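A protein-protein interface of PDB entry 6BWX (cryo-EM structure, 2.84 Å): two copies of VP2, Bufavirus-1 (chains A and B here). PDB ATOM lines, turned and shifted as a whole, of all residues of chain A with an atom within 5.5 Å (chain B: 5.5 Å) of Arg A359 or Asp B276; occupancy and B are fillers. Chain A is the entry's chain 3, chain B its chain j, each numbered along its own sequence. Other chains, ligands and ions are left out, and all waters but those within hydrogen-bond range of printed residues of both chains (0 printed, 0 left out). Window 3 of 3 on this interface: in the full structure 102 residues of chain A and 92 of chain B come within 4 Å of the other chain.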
ATOM      1  N   ILE A 346     -11.518  -6.097 -25.999  1.00  0.00           N
ATOM      2  CA  ILE A 346     -12.823  -6.726 -26.015  1.00  0.00           C
ATOM      3  C   ILE A 346     -13.166  -7.066 -27.459  1.00  0.00           C
ATOM      4  O   ILE A 346     -12.623  -6.485 -28.402  1.00  0.00           O
ATOM      5  CB  ILE A 346     -13.871  -5.799 -25.390  1.00  0.00           C
ATOM      6  CG1 ILE A 346     -13.325  -5.192 -24.103  1.00  0.00           C
ATOM      7  CG2 ILE A 346     -15.137  -6.560 -25.064  1.00  0.00           C
ATOM      8  CD1 ILE A 346     -12.932  -6.191 -23.083  1.00  0.00           C
ATOM      9  N   PHE A 347     -14.017  -8.067 -27.648  1.00  0.00           N
ATOM     10  CA  PHE A 347     -14.418  -8.379 -29.013  1.00  0.00           C
ATOM     11  C   PHE A 347     -15.706  -9.179 -29.017  1.00  0.00           C
ATOM     12  O   PHE A 347     -16.127  -9.731 -27.998  1.00  0.00           O
ATOM     13  CB  PHE A 347     -13.304  -9.096 -29.781  1.00  0.00           C
ATOM     14  CG  PHE A 347     -12.728 -10.266 -29.066  1.00  0.00           C
ATOM     15  CD1 PHE A 347     -11.679 -10.096 -28.188  1.00  0.00           C
ATOM     16  CD2 PHE A 347     -13.228 -11.533 -29.264  1.00  0.00           C
ATOM     17  CE1 PHE A 347     -11.145 -11.162 -27.524  1.00  0.00           C
ATOM     18  CE2 PHE A 347     -12.691 -12.606 -28.605  1.00  0.00           C
ATOM     19  CZ  PHE A 347     -11.648 -12.420 -27.733  1.00  0.00           C
ATOM     20  N   ASP A 348     -16.328  -9.219 -30.186  1.00  0.00           N
ATOM     21  CA  ASP A 348     -17.679  -9.711 -30.377  1.00  0.00           C
ATOM     22  C   ASP A 348     -17.657 -10.945 -31.278  1.00  0.00           C
ATOM     23  O   ASP A 348     -16.604 -11.407 -31.719  1.00  0.00           O
ATOM     24  CB  ASP A 348     -18.552  -8.599 -30.963  1.00  0.00           C
ATOM     25  CG  ASP A 348     -20.022  -8.931 -30.929  1.00  0.00           C
ATOM     26  OD1 ASP A 348     -20.372  -9.979 -30.349  1.00  0.00           O
ATOM     27  OD2 ASP A 348     -20.826  -8.157 -31.491  1.00  0.00           O
ATOM     28  N   ASP A 353     -15.202 -13.783 -31.282  1.00  0.00           N
ATOM     29  CA  ASP A 353     -15.760 -14.427 -30.107  1.00  0.00           C
ATOM     30  C   ASP A 353     -16.591 -15.622 -30.547  1.00  0.00           C
ATOM     31  O   ASP A 353     -17.245 -15.585 -31.592  1.00  0.00           O
ATOM     32  CB  ASP A 353     -16.624 -13.462 -29.303  1.00  0.00           C
ATOM     33  CG  ASP A 353     -17.104 -14.061 -28.008  1.00  0.00           C
ATOM     34  OD1 ASP A 353     -16.669 -15.176 -27.667  1.00  0.00           O
ATOM     35  OD2 ASP A 353     -17.926 -13.424 -27.328  1.00  0.00           O
ATOM     36  N   ASP A 355     -19.070 -17.145 -28.540  1.00  0.00           N
ATOM     37  CA  ASP A 355     -20.451 -17.038 -28.094  1.00  0.00           C
ATOM     38  C   ASP A 355     -21.170 -15.754 -28.468  1.00  0.00           C
ATOM     39  O   ASP A 355     -20.705 -14.664 -28.158  1.00  0.00           O
ATOM     40  CB  ASP A 355     -20.521 -17.226 -26.577  1.00  0.00           C
ATOM     41  CG  ASP A 355     -19.679 -18.387 -26.099  1.00  0.00           C
ATOM     42  OD1 ASP A 355     -18.946 -18.963 -26.928  1.00  0.00           O
ATOM     43  OD2 ASP A 355     -19.743 -18.723 -24.897  1.00  0.00           O
ATOM     44  N   ALA A 357     -24.012 -12.873 -28.263  1.00  0.00           N
ATOM     45  CA  ALA A 357     -24.577 -12.102 -27.140  1.00  0.00           C
ATOM     46  C   ALA A 357     -23.720 -12.103 -25.863  1.00  0.00           C
ATOM     47  O   ALA A 357     -24.231 -11.932 -24.760  1.00  0.00           O
ATOM     48  CB  ALA A 357     -26.037 -12.460 -26.847  1.00  0.00           C
ATOM     49  N   HIS A 358     -22.417 -12.295 -26.045  1.00  0.00           N
ATOM     50  CA  HIS A 358     -21.420 -12.274 -24.982  1.00  0.00           C
ATOM     51  C   HIS A 358     -20.130 -11.770 -25.612  1.00  0.00           C
ATOM     52  O   HIS A 358     -19.921 -11.942 -26.807  1.00  0.00           O
ATOM     53  CB  HIS A 358     -21.242 -13.644 -24.341  1.00  0.00           C
ATOM     54  CG  HIS A 358     -22.210 -13.910 -23.231  1.00  0.00           C
ATOM     55  ND1 HIS A 358     -23.434 -14.505 -23.440  1.00  0.00           N
ATOM     56  CD2 HIS A 358     -22.147 -13.630 -21.909  1.00  0.00           C
ATOM     57  CE1 HIS A 358     -24.078 -14.597 -22.291  1.00  0.00           C
ATOM     58  NE2 HIS A 358     -23.319 -14.072 -21.346  1.00  0.00           N
ATOM     59  N   ARG A 359     -19.247 -11.177 -24.821  1.00  0.00           N
ATOM     60  CA  ARG A 359     -18.034 -10.616 -25.400  1.00  0.00           C
ATOM     61  C   ARG A 359     -16.819 -11.170 -24.680  1.00  0.00           C
ATOM     62  O   ARG A 359     -16.642 -10.932 -23.482  1.00  0.00           O
ATOM     63  CB  ARG A 359     -18.047  -9.089 -25.333  1.00  0.00           C
ATOM     64  CG  ARG A 359     -19.024  -8.461 -26.288  1.00  0.00           C
ATOM     65  CD  ARG A 359     -19.018  -6.959 -26.191  1.00  0.00           C
ATOM     66  NE  ARG A 359     -19.869  -6.371 -27.216  1.00  0.00           N
ATOM     67  CZ  ARG A 359     -21.185  -6.235 -27.109  1.00  0.00           C
ATOM     68  NH1 ARG A 359     -21.809  -6.642 -26.014  1.00  0.00           N
ATOM     69  NH2 ARG A 359     -21.876  -5.691 -28.098  1.00  0.00           N
ATOM     70  N   ASP A 360     -15.998 -11.917 -25.406  1.00  0.00           N
ATOM     71  CA  ASP A 360     -14.754 -12.432 -24.867  1.00  0.00           C
ATOM     72  C   ASP A 360     -13.687 -11.338 -24.855  1.00  0.00           C
ATOM     73  O   ASP A 360     -13.793 -10.323 -25.545  1.00  0.00           O
ATOM     74  CB  ASP A 360     -14.284 -13.639 -25.672  1.00  0.00           C
ATOM     75  CG  ASP A 360     -13.187 -14.409 -24.973  1.00  0.00           C
ATOM     76  OD1 ASP A 360     -12.840 -14.044 -23.832  1.00  0.00           O
ATOM     77  OD2 ASP A 360     -12.685 -15.391 -25.550  1.00  0.00           O
ATOM     78  N   GLN A 361     -12.652 -11.559 -24.048  1.00  0.00           N
ATOM     79  CA  GLN A 361     -11.623 -10.571 -23.764  1.00  0.00           C
ATOM     80  C   GLN A 361     -10.255 -11.188 -24.021  1.00  0.00           C
ATOM     81  O   GLN A 361     -10.120 -12.406 -24.140  1.00  0.00           O
ATOM     82  CB  GLN A 361     -11.730 -10.117 -22.312  1.00  0.00           C
ATOM     83  CG  GLN A 361     -13.082  -9.561 -21.983  1.00  0.00           C
ATOM     84  CD  GLN A 361     -13.252  -9.310 -20.514  1.00  0.00           C
ATOM     85  OE1 GLN A 361     -12.557  -9.898 -19.690  1.00  0.00           O
ATOM     86  NE2 GLN A 361     -14.198  -8.453 -20.171  1.00  0.00           N
ATOM     87  N   ILE B 274     -23.409   3.989 -24.881  1.00  0.00           N
ATOM     88  CA  ILE B 274     -23.732   2.571 -24.848  1.00  0.00           C
ATOM     89  C   ILE B 274     -22.945   1.898 -23.733  1.00  0.00           C
ATOM     90  O   ILE B 274     -21.742   2.129 -23.568  1.00  0.00           O
ATOM     91  CB  ILE B 274     -23.438   1.920 -26.206  1.00  0.00           C
ATOM     92  CG1 ILE B 274     -24.160   2.671 -27.318  1.00  0.00           C
ATOM     93  CG2 ILE B 274     -23.881   0.481 -26.198  1.00  0.00           C
ATOM     94  CD1 ILE B 274     -25.639   2.718 -27.140  1.00  0.00           C
ATOM     95  N   ARG B 275     -23.627   1.058 -22.957  1.00  0.00           N
ATOM     96  CA  ARG B 275     -22.998   0.452 -21.791  1.00  0.00           C
ATOM     97  C   ARG B 275     -21.977  -0.605 -22.182  1.00  0.00           C
ATOM     98  O   ARG B 275     -20.844  -0.587 -21.689  1.00  0.00           O
ATOM     99  CB  ARG B 275     -24.058  -0.168 -20.888  1.00  0.00           C
ATOM    100  CG  ARG B 275     -25.095   0.806 -20.389  1.00  0.00           C
ATOM    101  CD  ARG B 275     -24.486   1.832 -19.463  1.00  0.00           C
ATOM    102  NE  ARG B 275     -25.488   2.761 -18.947  1.00  0.00           N
ATOM    103  CZ  ARG B 275     -26.225   2.538 -17.864  1.00  0.00           C
ATOM    104  NH1 ARG B 275     -27.113   3.439 -17.467  1.00  0.00           N
ATOM    105  NH2 ARG B 275     -26.073   1.415 -17.175  1.00  0.00           N
ATOM    106  N   ASP B 276     -22.355  -1.531 -23.057  1.00  0.00           N
ATOM    107  CA  ASP B 276     -21.543  -2.702 -23.370  1.00  0.00           C
ATOM    108  C   ASP B 276     -21.064  -2.595 -24.811  1.00  0.00           C
ATOM    109  O   ASP B 276     -21.855  -2.753 -25.744  1.00  0.00           O
ATOM    110  CB  ASP B 276     -22.347  -3.980 -23.152  1.00  0.00           C
ATOM    111  CG  ASP B 276     -21.502  -5.229 -23.271  1.00  0.00           C
ATOM    112  OD1 ASP B 276     -20.269  -5.110 -23.428  1.00  0.00           O
ATOM    113  OD2 ASP B 276     -22.075  -6.338 -23.210  1.00  0.00           O
ATOM    114  N   ILE B 277     -19.766  -2.350 -24.989  1.00  0.00           N
ATOM    115  CA  ILE B 277     -19.161  -2.219 -26.306  1.00  0.00           C
ATOM    116  C   ILE B 277     -17.867  -3.018 -26.335  1.00  0.00           C
ATOM    117  O   ILE B 277     -17.288  -3.352 -25.301  1.00  0.00           O
ATOM    118  CB  ILE B 277     -18.888  -0.754 -26.683  1.00  0.00           C
ATOM    119  CG1 ILE B 277     -17.945  -0.130 -25.669  1.00  0.00           C
ATOM    120  CG2 ILE B 277     -20.177   0.027 -26.745  1.00  0.00           C
ATOM    121  CD1 ILE B 277     -17.451   1.206 -26.079  1.00  0.00           C
ATOM    122  N   ASN B 278     -17.429  -3.339 -27.546  1.00  0.00           N
ATOM    123  CA  ASN B 278     -16.394  -4.335 -27.779  1.00  0.00           C
ATOM    124  C   ASN B 278     -14.997  -3.761 -28.011  1.00  0.00           C
ATOM    125  O   ASN B 278     -14.127  -4.489 -28.477  1.00  0.00           O
ATOM    126  CB  ASN B 278     -16.792  -5.245 -28.940  1.00  0.00           C
ATOM    127  CG  ASN B 278     -16.937  -4.503 -30.229  1.00  0.00           C
ATOM    128  OD1 ASN B 278     -16.988  -3.277 -30.243  1.00  0.00           O
ATOM    129  ND2 ASN B 278     -17.012  -5.238 -31.326  1.00  0.00           N
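Of the 5 printed residues of chain B, 3 touch a printed residue of chain A.
Among the printed residues, Asp or Glu carboxylates within 4 Å of a Lys or Arg side-chain nitrogen of the other chain: Arg A359 with Asp B276 (2.8 Å).
Among the printed residues, merely in contact across the chains: Phe A347 with Asn B278, Arg A359 with Asn B278, Asp A348 with Asn B278 and Ile A346 with Ile B277.
No position is printed for both chains.
Printed residues of chain B within 4 Å of Asp A348: Asn B278.
Asp A355 touches none of the printed residues of chain B.
Of the printed residues of chain B, Arg A359 touches Asp B276 and Asn B278.
Ile B274 touches none of the printed residues of chain A.
Of the printed residues of chain A, Ile B277 touches Ile A346.
Printed residues of chain A within 4 Å of Asn B278: Ile A346 (2.5 Å), Phe A347 (3.7 Å), Asp A348 (3.7 Å) and Arg A359 (3.7 Å).
O of Ile A346 lies close to O of Asn B278 (2.5 Å).
The side-chain carboxylate (OD2) of Asp B276 is in salt-bridge range of the guanidinium group (NH1) of Arg A359 (2.8 Å).
The backbone NH (N) of Phe A347 is in hydrogen-bond range of the backbone carbonyl oxygen (O) of Asp A360 (3.1 Å).
N of Asp A353 lies within hydrogen-bond range of O of Asp A348.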
